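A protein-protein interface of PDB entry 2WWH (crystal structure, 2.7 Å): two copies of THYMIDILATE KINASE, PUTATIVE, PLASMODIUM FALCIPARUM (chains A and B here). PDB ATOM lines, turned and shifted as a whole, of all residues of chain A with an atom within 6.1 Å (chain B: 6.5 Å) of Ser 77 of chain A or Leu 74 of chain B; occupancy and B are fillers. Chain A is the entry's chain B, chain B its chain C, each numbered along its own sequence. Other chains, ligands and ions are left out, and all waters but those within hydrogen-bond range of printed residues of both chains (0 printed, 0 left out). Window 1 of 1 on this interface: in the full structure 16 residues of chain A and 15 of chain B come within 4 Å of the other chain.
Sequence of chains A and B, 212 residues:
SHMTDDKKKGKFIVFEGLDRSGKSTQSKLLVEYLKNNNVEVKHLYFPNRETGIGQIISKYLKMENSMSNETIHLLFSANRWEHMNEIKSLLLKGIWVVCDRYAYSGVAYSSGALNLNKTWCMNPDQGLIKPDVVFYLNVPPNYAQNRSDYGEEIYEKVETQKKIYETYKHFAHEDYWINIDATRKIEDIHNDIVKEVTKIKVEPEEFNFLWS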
ATOM      1  N   ILE A  57      -5.299  -4.408  -6.149  1.00  0.00           N
ATOM      2  CA  ILE A  57      -6.162  -4.210  -4.988  1.00  0.00           C
ATOM      3  C   ILE A  57      -6.199  -5.509  -4.205  1.00  0.00           C
ATOM      4  O   ILE A  57      -5.839  -5.530  -3.042  1.00  0.00           O
ATOM      5  CB  ILE A  57      -7.589  -3.760  -5.343  1.00  0.00           C
ATOM      6  CG1 ILE A  57      -7.575  -2.377  -5.981  1.00  0.00           C
ATOM      7  CG2 ILE A  57      -8.392  -3.651  -4.117  1.00  0.00           C
ATOM      8  CD1 ILE A  57      -8.811  -2.034  -6.741  1.00  0.00           C
ATOM      9  N   ILE A  72      -3.415   3.195  -2.777  1.00  0.00           N
ATOM     10  CA  ILE A  72      -4.466   2.209  -2.783  1.00  0.00           C
ATOM     11  C   ILE A  72      -5.828   2.862  -2.954  1.00  0.00           C
ATOM     12  O   ILE A  72      -6.743   2.257  -3.538  1.00  0.00           O
ATOM     13  CB  ILE A  72      -4.450   1.343  -1.552  1.00  0.00           C
ATOM     14  CG1 ILE A  72      -5.464   0.213  -1.716  1.00  0.00           C
ATOM     15  CG2 ILE A  72      -4.723   2.162  -0.308  1.00  0.00           C
ATOM     16  CD1 ILE A  72      -5.266  -0.643  -2.947  1.00  0.00           C
ATOM     17  N   HIS A  73      -5.960   4.104  -2.483  1.00  0.00           N
ATOM     18  CA  HIS A  73      -7.232   4.762  -2.536  1.00  0.00           C
ATOM     19  C   HIS A  73      -7.585   5.033  -3.990  1.00  0.00           C
ATOM     20  O   HIS A  73      -8.739   4.852  -4.401  1.00  0.00           O
ATOM     21  CB  HIS A  73      -7.241   6.050  -1.736  1.00  0.00           C
ATOM     22  CG  HIS A  73      -8.527   6.808  -1.871  1.00  0.00           C
ATOM     23  ND1 HIS A  73      -9.644   6.520  -1.117  1.00  0.00           N
ATOM     24  CD2 HIS A  73      -8.893   7.794  -2.720  1.00  0.00           C
ATOM     25  CE1 HIS A  73     -10.632   7.310  -1.477  1.00  0.00           C
ATOM     26  NE2 HIS A  73     -10.200   8.099  -2.441  1.00  0.00           N
ATOM     27  N   LEU A  74      -6.590   5.443  -4.768  1.00  0.00           N
ATOM     28  CA  LEU A  74      -6.828   5.819  -6.144  1.00  0.00           C
ATOM     29  C   LEU A  74      -7.060   4.599  -7.010  1.00  0.00           C
ATOM     30  O   LEU A  74      -7.862   4.665  -7.942  1.00  0.00           O
ATOM     31  CB  LEU A  74      -5.696   6.678  -6.684  1.00  0.00           C
ATOM     32  CG  LEU A  74      -5.552   7.990  -5.924  1.00  0.00           C
ATOM     33  CD1 LEU A  74      -4.293   8.692  -6.340  1.00  0.00           C
ATOM     34  CD2 LEU A  74      -6.766   8.863  -6.119  1.00  0.00           C
ATOM     35  N   LEU A  75      -6.395   3.482  -6.699  1.00  0.00           N
ATOM     36  CA  LEU A  75      -6.722   2.225  -7.370  1.00  0.00           C
ATOM     37  C   LEU A  75      -8.208   1.851  -7.218  1.00  0.00           C
ATOM     38  O   LEU A  75      -8.869   1.523  -8.191  1.00  0.00           O
ATOM     39  CB  LEU A  75      -5.833   1.085  -6.881  1.00  0.00           C
ATOM     40  CG  LEU A  75      -4.321   1.095  -7.191  1.00  0.00           C
ATOM     41  CD1 LEU A  75      -3.617  -0.200  -6.703  1.00  0.00           C
ATOM     42  CD2 LEU A  75      -4.031   1.306  -8.650  1.00  0.00           C
ATOM     43  N   PHE A  76      -8.729   1.911  -5.993  1.00  0.00           N
ATOM     44  CA  PHE A  76     -10.130   1.557  -5.719  1.00  0.00           C
ATOM     45  C   PHE A  76     -11.106   2.361  -6.577  1.00  0.00           C
ATOM     46  O   PHE A  76     -12.175   1.866  -6.971  1.00  0.00           O
ATOM     47  CB  PHE A  76     -10.462   1.834  -4.268  1.00  0.00           C
ATOM     48  CG  PHE A  76     -10.142   0.717  -3.350  1.00  0.00           C
ATOM     49  CD1 PHE A  76     -10.802  -0.504  -3.466  1.00  0.00           C
ATOM     50  CD2 PHE A  76      -9.225   0.893  -2.331  1.00  0.00           C
ATOM     51  CE1 PHE A  76     -10.528  -1.539  -2.600  1.00  0.00           C
ATOM     52  CE2 PHE A  76      -8.941  -0.136  -1.465  1.00  0.00           C
ATOM     53  CZ  PHE A  76      -9.593  -1.363  -1.603  1.00  0.00           C
ATOM     54  N   SER A  77     -10.718   3.602  -6.842  1.00  0.00           N
ATOM     55  CA  SER A  77     -11.504   4.529  -7.602  1.00  0.00           C
ATOM     56  C   SER A  77     -11.350   4.248  -9.099  1.00  0.00           C
ATOM     57  O   SER A  77     -12.298   4.379  -9.858  1.00  0.00           O
ATOM     58  CB  SER A  77     -11.067   5.949  -7.260  1.00  0.00           C
ATOM     59  OG  SER A  77     -11.734   6.890  -8.061  1.00  0.00           O
ATOM     60  N   ALA A  78     -10.157   3.863  -9.527  1.00  0.00           N
ATOM     61  CA  ALA A  78      -9.905   3.655 -10.933  1.00  0.00           C
ATOM     62  C   ALA A  78     -10.667   2.408 -11.345  1.00  0.00           C
ATOM     63  O   ALA A  78     -11.258   2.363 -12.429  1.00  0.00           O
ATOM     64  CB  ALA A  78      -8.417   3.497 -11.175  1.00  0.00           C
ATOM     65  N   ASN A  79     -10.657   1.417 -10.454  1.00  0.00           N
ATOM     66  CA  ASN A  79     -11.441   0.173 -10.563  1.00  0.00           C
ATOM     67  C   ASN A  79     -12.963   0.365 -10.834  1.00  0.00           C
ATOM     68  O   ASN A  79     -13.606  -0.425 -11.510  1.00  0.00           O
ATOM     69  CB  ASN A  79     -11.250  -0.616  -9.274  1.00  0.00           C
ATOM     70  CG  ASN A  79     -11.617  -2.074  -9.412  1.00  0.00           C
ATOM     71  OD1 ASN A  79     -12.231  -2.640  -8.519  1.00  0.00           O
ATOM     72  ND2 ASN A  79     -11.236  -2.696 -10.518  1.00  0.00           N
ATOM     73  N   ARG A  80     -13.521   1.433 -10.294  1.00  0.00           N
ATOM     74  CA  ARG A  80     -14.879   1.792 -10.572  1.00  0.00           C
ATOM     75  C   ARG A  80     -14.989   2.460 -11.937  1.00  0.00           C
ATOM     76  O   ARG A  80     -15.967   2.234 -12.652  1.00  0.00           O
ATOM     77  CB  ARG A  80     -15.409   2.713  -9.470  1.00  0.00           C
ATOM     78  CG  ARG A  80     -15.790   1.975  -8.181  1.00  0.00           C
ATOM     79  CD  ARG A  80     -16.358   2.907  -7.127  1.00  0.00           C
ATOM     80  NE  ARG A  80     -15.349   3.731  -6.445  1.00  0.00           N
ATOM     81  CZ  ARG A  80     -14.581   3.275  -5.453  1.00  0.00           C
ATOM     82  NH1 ARG A  80     -14.673   1.986  -5.093  1.00  0.00           N
ATOM     83  NH2 ARG A  80     -13.702   4.073  -4.847  1.00  0.00           N
ATOM     84  N   TRP A  81     -14.021   3.294 -12.316  1.00  0.00           N
ATOM     85  CA  TRP A  81     -14.109   3.959 -13.636  1.00  0.00           C
ATOM     86  C   TRP A  81     -13.896   2.949 -14.805  1.00  0.00           C
ATOM     87  O   TRP A  81     -14.578   3.021 -15.834  1.00  0.00           O
ATOM     88  CB  TRP A  81     -13.144   5.154 -13.761  1.00  0.00           C
ATOM     89  CG  TRP A  81     -13.411   6.354 -12.887  1.00  0.00           C
ATOM     90  CD1 TRP A  81     -12.862   6.611 -11.655  1.00  0.00           C
ATOM     91  CD2 TRP A  81     -14.235   7.484 -13.189  1.00  0.00           C
ATOM     92  NE1 TRP A  81     -13.301   7.816 -11.171  1.00  0.00           N
ATOM     93  CE2 TRP A  81     -14.146   8.375 -12.091  1.00  0.00           C
ATOM     94  CE3 TRP A  81     -15.056   7.826 -14.271  1.00  0.00           C
ATOM     95  CZ2 TRP A  81     -14.840   9.591 -12.053  1.00  0.00           C
ATOM     96  CZ3 TRP A  81     -15.758   9.015 -14.230  1.00  0.00           C
ATOM     97  CH2 TRP A  81     -15.646   9.888 -13.132  1.00  0.00           C
ATOM     98  N   GLU A  82     -12.970   2.007 -14.646  1.00  0.00           N
ATOM     99  CA  GLU A  82     -12.807   0.961 -15.667  1.00  0.00           C
ATOM    100  C   GLU A  82     -14.112   0.173 -15.894  1.00  0.00           C
ATOM    101  O   GLU A  82     -14.204  -0.650 -16.784  1.00  0.00           O
ATOM    102  CB  GLU A  82     -11.598   0.025 -15.392  1.00  0.00           C
ATOM    103  CG  GLU A  82     -11.598  -0.747 -14.091  1.00  0.00           C
ATOM    104  CD  GLU A  82     -10.435  -1.748 -13.985  1.00  0.00           C
ATOM    105  OE1 GLU A  82      -9.946  -2.218 -15.026  1.00  0.00           O
ATOM    106  OE2 GLU A  82     -10.004  -2.086 -12.860  1.00  0.00           O
ATOM    107  N   PRO A 124     -11.635  11.822  -6.583  1.00  0.00           N
ATOM    108  CA  PRO A 124     -11.480  10.926  -7.729  1.00  0.00           C
ATOM    109  C   PRO A 124     -12.809  10.279  -8.201  1.00  0.00           C
ATOM    110  O   PRO A 124     -12.977  10.043  -9.399  1.00  0.00           O
ATOM    111  CB  PRO A 124     -10.506   9.852  -7.204  1.00  0.00           C
ATOM    112  CG  PRO A 124     -10.695   9.870  -5.752  1.00  0.00           C
ATOM    113  CD  PRO A 124     -10.883  11.313  -5.419  1.00  0.00           C
ATOM    114  N   ASP A 125     -13.729  10.001  -7.279  1.00  0.00           N
ATOM    115  CA  ASP A 125     -14.955   9.292  -7.624  1.00  0.00           C
ATOM    116  C   ASP A 125     -16.056  10.234  -8.159  1.00  0.00           C
ATOM    117  O   ASP A 125     -17.159   9.775  -8.487  1.00  0.00           O
ATOM    118  CB  ASP A 125     -15.481   8.488  -6.433  1.00  0.00           C
ATOM    119  CG  ASP A 125     -14.764   7.144  -6.242  1.00  0.00           C
ATOM    120  OD1 ASP A 125     -14.231   6.527  -7.203  1.00  0.00           O
ATOM    121  OD2 ASP A 125     -14.758   6.662  -5.092  1.00  0.00           O
ATOM    122  N   LEU A 128     -18.605   9.581 -11.483  1.00  0.00           N
ATOM    123  CA  LEU A 128     -19.145   8.234 -11.505  1.00  0.00           C
ATOM    124  C   LEU A 128     -20.657   8.352 -11.533  1.00  0.00           C
ATOM    125  O   LEU A 128     -21.193   9.390 -11.137  1.00  0.00           O
ATOM    126  CB  LEU A 128     -18.733   7.480 -10.247  1.00  0.00           C
ATOM    127  CG  LEU A 128     -17.261   7.089 -10.125  1.00  0.00           C
ATOM    128  CD1 LEU A 128     -17.111   6.101  -8.969  1.00  0.00           C
ATOM    129  CD2 LEU A 128     -16.738   6.503 -11.444  1.00  0.00           C
ATOM    130  N   ILE B  53       1.544  -0.822 -11.452  1.00  0.00           N
ATOM    131  CA  ILE B  53       0.761   0.236 -12.065  1.00  0.00           C
ATOM    132  C   ILE B  53       1.398   0.777 -13.350  1.00  0.00           C
ATOM    133  O   ILE B  53       0.733   0.929 -14.376  1.00  0.00           O
ATOM    134  CB  ILE B  53       0.532   1.393 -11.072  1.00  0.00           C
ATOM    135  CG1 ILE B  53      -0.212   0.882  -9.819  1.00  0.00           C
ATOM    136  CG2 ILE B  53      -0.214   2.537 -11.742  1.00  0.00           C
ATOM    137  CD1 ILE B  53      -0.249   1.853  -8.701  1.00  0.00           C
ATOM    138  N   ASN B  69     -10.652   7.394 -19.968  1.00  0.00           N
ATOM    139  CA  ASN B  69      -9.794   8.515 -19.618  1.00  0.00           C
ATOM    140  C   ASN B  69      -9.575   8.542 -18.129  1.00  0.00           C
ATOM    141  O   ASN B  69      -8.433   8.573 -17.678  1.00  0.00           O
ATOM    142  CB  ASN B  69     -10.391   9.844 -20.061  1.00  0.00           C
ATOM    143  CG  ASN B  69     -10.734   9.871 -21.548  1.00  0.00           C
ATOM    144  OD1 ASN B  69     -11.823  10.294 -21.917  1.00  0.00           O
ATOM    145  ND2 ASN B  69      -9.826   9.394 -22.396  1.00  0.00           N
ATOM    146  N   GLU B  70     -10.660   8.490 -17.354  1.00  0.00           N
ATOM    147  CA  GLU B  70     -10.522   8.588 -15.909  1.00  0.00           C
ATOM    148  C   GLU B  70      -9.714   7.431 -15.324  1.00  0.00           C
ATOM    149  O   GLU B  70      -8.863   7.664 -14.462  1.00  0.00           O
ATOM    150  CB  GLU B  70     -11.873   8.744 -15.207  1.00  0.00           C
ATOM    151  CG  GLU B  70     -12.657  10.017 -15.568  1.00  0.00           C
ATOM    152  CD  GLU B  70     -13.482   9.877 -16.830  1.00  0.00           C
ATOM    153  OE1 GLU B  70     -13.483   8.772 -17.454  1.00  0.00           O
ATOM    154  OE2 GLU B  70     -14.130  10.886 -17.198  1.00  0.00           O
ATOM    155  N   THR B  71      -9.947   6.196 -15.785  1.00  0.00           N
ATOM    156  CA  THR B  71      -9.121   5.077 -15.323  1.00  0.00           C
ATOM    157  C   THR B  71      -7.628   5.459 -15.403  1.00  0.00           C
ATOM    158  O   THR B  71      -6.871   5.247 -14.457  1.00  0.00           O
ATOM    159  CB  THR B  71      -9.338   3.757 -16.135  1.00  0.00           C
ATOM    160  OG1 THR B  71     -10.731   3.504 -16.377  1.00  0.00           O
ATOM    161  CG2 THR B  71      -8.760   2.577 -15.399  1.00  0.00           C
ATOM    162  N   ILE B  72      -7.201   6.035 -16.526  1.00  0.00           N
ATOM    163  CA  ILE B  72      -5.764   6.131 -16.801  1.00  0.00           C
ATOM    164  C   ILE B  72      -5.163   7.267 -15.981  1.00  0.00           C
ATOM    165  O   ILE B  72      -4.057   7.138 -15.407  1.00  0.00           O
ATOM    166  CB  ILE B  72      -5.412   6.218 -18.353  1.00  0.00           C
ATOM    167  CG1 ILE B  72      -3.913   6.385 -18.597  1.00  0.00           C
ATOM    168  CG2 ILE B  72      -6.156   7.334 -19.052  1.00  0.00           C
ATOM    169  CD1 ILE B  72      -3.065   5.218 -18.122  1.00  0.00           C
ATOM    170  N   HIS B  73      -5.913   8.364 -15.918  1.00  0.00           N
ATOM    171  CA  HIS B  73      -5.478   9.531 -15.215  1.00  0.00           C
ATOM    172  C   HIS B  73      -5.205   9.235 -13.735  1.00  0.00           C
ATOM    173  O   HIS B  73      -4.169   9.636 -13.201  1.00  0.00           O
ATOM    174  CB  HIS B  73      -6.500  10.631 -15.345  1.00  0.00           C
ATOM    175  CG  HIS B  73      -6.117  11.867 -14.610  1.00  0.00           C
ATOM    176  ND1 HIS B  73      -5.322  12.845 -15.168  1.00  0.00           N
ATOM    177  CD2 HIS B  73      -6.384  12.273 -13.347  1.00  0.00           C
ATOM    178  CE1 HIS B  73      -5.146  13.817 -14.291  1.00  0.00           C
ATOM    179  NE2 HIS B  73      -5.773  13.490 -13.174  1.00  0.00           N
ATOM    180  N   LEU B  74      -6.111   8.528 -13.073  1.00  0.00           N
ATOM    181  CA  LEU B  74      -5.850   8.144 -11.698  1.00  0.00           C
ATOM    182  C   LEU B  74      -4.651   7.189 -11.606  1.00  0.00           C
ATOM    183  O   LEU B  74      -3.902   7.257 -10.636  1.00  0.00           O
ATOM    184  CB  LEU B  74      -7.100   7.581 -11.019  1.00  0.00           C
ATOM    185  CG  LEU B  74      -8.365   8.459 -11.101  1.00  0.00           C
ATOM    186  CD1 LEU B  74      -9.639   7.671 -10.691  1.00  0.00           C
ATOM    187  CD2 LEU B  74      -8.240   9.749 -10.301  1.00  0.00           C
ATOM    188  N   LEU B  75      -4.429   6.336 -12.610  1.00  0.00           N
ATOM    189  CA  LEU B  75      -3.220   5.501 -12.573  1.00  0.00           C
ATOM    190  C   LEU B  75      -1.940   6.331 -12.614  1.00  0.00           C
ATOM    191  O   LEU B  75      -0.983   6.023 -11.919  1.00  0.00           O
ATOM    192  CB  LEU B  75      -3.198   4.444 -13.665  1.00  0.00           C
ATOM    193  CG  LEU B  75      -4.293   3.373 -13.626  1.00  0.00           C
ATOM    194  CD1 LEU B  75      -4.012   2.251 -14.651  1.00  0.00           C
ATOM    195  CD2 LEU B  75      -4.517   2.768 -12.227  1.00  0.00           C
ATOM    196  N   PHE B  76      -1.930   7.402 -13.405  1.00  0.00           N
ATOM    197  CA  PHE B  76      -0.740   8.257 -13.499  1.00  0.00           C
ATOM    198  C   PHE B  76      -0.490   8.866 -12.131  1.00  0.00           C
ATOM    199  O   PHE B  76       0.640   8.866 -11.644  1.00  0.00           O
ATOM    200  CB  PHE B  76      -0.930   9.369 -14.530  1.00  0.00           C
ATOM    201  CG  PHE B  76      -0.517   8.998 -15.930  1.00  0.00           C
ATOM    202  CD1 PHE B  76       0.816   8.828 -16.260  1.00  0.00           C
ATOM    203  CD2 PHE B  76      -1.469   8.845 -16.934  1.00  0.00           C
ATOM    204  CE1 PHE B  76       1.198   8.507 -17.562  1.00  0.00           C
ATOM    205  CE2 PHE B  76      -1.094   8.520 -18.234  1.00  0.00           C
ATOM    206  CZ  PHE B  76       0.240   8.352 -18.546  1.00  0.00           C
ATOM    207  N   SER B  77      -1.559   9.352 -11.501  1.00  0.00           N
ATOM    208  CA  SER B  77      -1.468   9.842 -10.148  1.00  0.00           C
ATOM    209  C   SER B  77      -1.008   8.770  -9.152  1.00  0.00           C
ATOM    210  O   SER B  77      -0.126   9.000  -8.314  1.00  0.00           O
ATOM    211  CB  SER B  77      -2.799  10.397  -9.715  1.00  0.00           C
ATOM    212  OG  SER B  77      -2.605  11.484  -8.838  1.00  0.00           O
ATOM    213  N   ALA B  78      -1.605   7.588  -9.231  1.00  0.00           N
ATOM    214  CA  ALA B  78      -1.326   6.571  -8.244  1.00  0.00           C
ATOM    215  C   ALA B  78       0.157   6.367  -8.267  1.00  0.00           C
ATOM    216  O   ALA B  78       0.798   6.324  -7.222  1.00  0.00           O
ATOM    217  CB  ALA B  78      -2.027   5.327  -8.578  1.00  0.00           C
ATOM    218  N   ASN B  79       0.685   6.303  -9.488  1.00  0.00           N
ATOM    219  CA  ASN B  79       2.070   5.967  -9.783  1.00  0.00           C
ATOM    220  C   ASN B  79       3.042   6.917  -9.103  1.00  0.00           C
ATOM    221  O   ASN B  79       4.135   6.508  -8.718  1.00  0.00           O
ATOM    222  CB  ASN B  79       2.256   5.998 -11.301  1.00  0.00           C
ATOM    223  CG  ASN B  79       3.599   5.458 -11.759  1.00  0.00           C
ATOM    224  OD1 ASN B  79       4.228   6.049 -12.629  1.00  0.00           O
ATOM    225  ND2 ASN B  79       4.026   4.321 -11.210  1.00  0.00           N
ATOM    226  N   TRP B 120     -10.642  18.669 -11.581  1.00  0.00           N
ATOM    227  CA  TRP B 120     -10.745  17.229 -11.404  1.00  0.00           C
ATOM    228  C   TRP B 120      -9.403  16.539 -11.666  1.00  0.00           C
ATOM    229  O   TRP B 120      -9.060  15.564 -10.989  1.00  0.00           O
ATOM    230  CB  TRP B 120     -11.854  16.651 -12.296  1.00  0.00           C
ATOM    231  CG  TRP B 120     -12.205  15.210 -11.974  1.00  0.00           C
ATOM    232  CD1 TRP B 120     -13.242  14.776 -11.205  1.00  0.00           C
ATOM    233  CD2 TRP B 120     -11.523  14.026 -12.422  1.00  0.00           C
ATOM    234  NE1 TRP B 120     -13.247  13.404 -11.137  1.00  0.00           N
ATOM    235  CE2 TRP B 120     -12.203  12.920 -11.877  1.00  0.00           C
ATOM    236  CE3 TRP B 120     -10.403  13.793 -13.233  1.00  0.00           C
ATOM    237  CZ2 TRP B 120     -11.799  11.607 -12.107  1.00  0.00           C
ATOM    238  CZ3 TRP B 120     -10.007  12.483 -13.469  1.00  0.00           C
ATOM    239  CH2 TRP B 120     -10.695  11.408 -12.894  1.00  0.00           C
ATOM    240  N   PRO B 124      -6.340  14.614  -7.575  1.00  0.00           N
ATOM    241  CA  PRO B 124      -5.726  13.433  -7.020  1.00  0.00           C
ATOM    242  C   PRO B 124      -4.254  13.661  -6.754  1.00  0.00           C
ATOM    243  O   PRO B 124      -3.659  12.949  -5.960  1.00  0.00           O
ATOM    244  CB  PRO B 124      -5.911  12.405  -8.121  1.00  0.00           C
ATOM    245  CG  PRO B 124      -5.897  13.208  -9.366  1.00  0.00           C
ATOM    246  CD  PRO B 124      -6.657  14.440  -9.003  1.00  0.00           C
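N of Glu 82 of chain A sits at hydrogen-bond distance from OG1 of Thr 71 of chain B (3.2 Å).
The backbone carbonyl oxygen of Pro 124 of chain A lies within hydrogen-bond range of the indole nitrogen of Trp 81 of chain A (2.9 Å). The side-chain amide nitrogen (ND2) of Asn 79 of chain A sits at hydrogen-bond distance from the side-chain carboxylate (OE2) of Glu 82 of chain A (2.7 Å). The side-chain hydroxyl (OG) of Ser 77 of chain A is in hydrogen-bond range of the side-chain carboxylate (OD1) of Asp 125 of chain A.
Ile 53 of chain B touches Leu 75 of chain A (CD1 to CD2, 3.8 Å). Leu 75 of chain A touches Leu 75 of chain B. Ser 77 of chain A touches Leu 74 of chain B. O of Ala 78 of chain A touches CG2 of Thr 71 of chain B (3.9 Å). CB of Glu 70 of chain B touches CD2 of Trp 81 of chain A, at 3.4 Å. Thr 71 of chain B touches Trp 81 of chain A (OG1 to C, 3.6 Å). Trp 81 of chain A touches Leu 74 of chain B. CZ2 of Trp 81 of chain A touches CZ2 of Trp 120 of chain B (3.6 Å). Pro 124 of chain A touches Leu 74 of chain B. Pro 124 of chain A touches Trp 120 of chain B.
Of chain B, only Leu 74 (3.5 Å) comes within 4 Å of Ser 77 of chain A. Of the printed residues of chain B, Glu 82 of chain A touches Thr 71 (3.2 Å). Printed residues of chain B within 4 Å of Trp 81 of chain A: Glu 70 (3.4 Å), Thr 71 (3.6 Å), Leu 74 (3.5 Å) and Trp 120 (3.6 Å). His 73 of chain B touches none of the printed residues of chain A. The nearest residue of chain B that does not touch Ser 77 of chain A is Trp 120 of chain B (6.2 Å). The nearest printed residue of chain A that does not touch Ile 53 of chain B is Ile 72 of chain A (6.8 Å).
Of the 14 printed residues of chain B, 6 touch a printed residue of chain A. Hydrophobic or aromatic side chains of chain B within 4 Å of the printed part of chain A: Ile 53, Leu 74, Leu 75 and Trp 120. Along chain B the printed residues that touch a printed residue of chain A span positions 53 to 120. Hydrophobic or aromatic side chains of chain A within 4 Å of the printed part of chain B: Leu 75, Trp 81 and Pro 124. Along chain A the printed residues that touch a printed residue of chain B span positions 75 to 124. Among the printed residues, 11 pairs touch across the chains. Among the printed residues, no Asp or Glu carboxylate lies within 4 Å of a Lys or Arg side-chain nitrogen of the other chain.
Leu 75 of chain A touches its own counterpart, Leu 75 of chain B. Ser 77 of chain A touches Leu 74 of chain B, but with the chains exchanged Leu 74 of chain A does not touch Ser 77 of chain B (4.1 Å). Pro 124 of chain A touches Leu 74 of chain B, but with the chains exchanged Leu 74 of chain A does not touch Pro 124 of chain B (4.2 Å). Positions printed for both chains: 72, 73, 74, 75, 76, 77, 78, 79 and 124. Of the 11 pairs that touch across the chains among the printed residues, 1 has its exchanged pair printed and touching as well.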
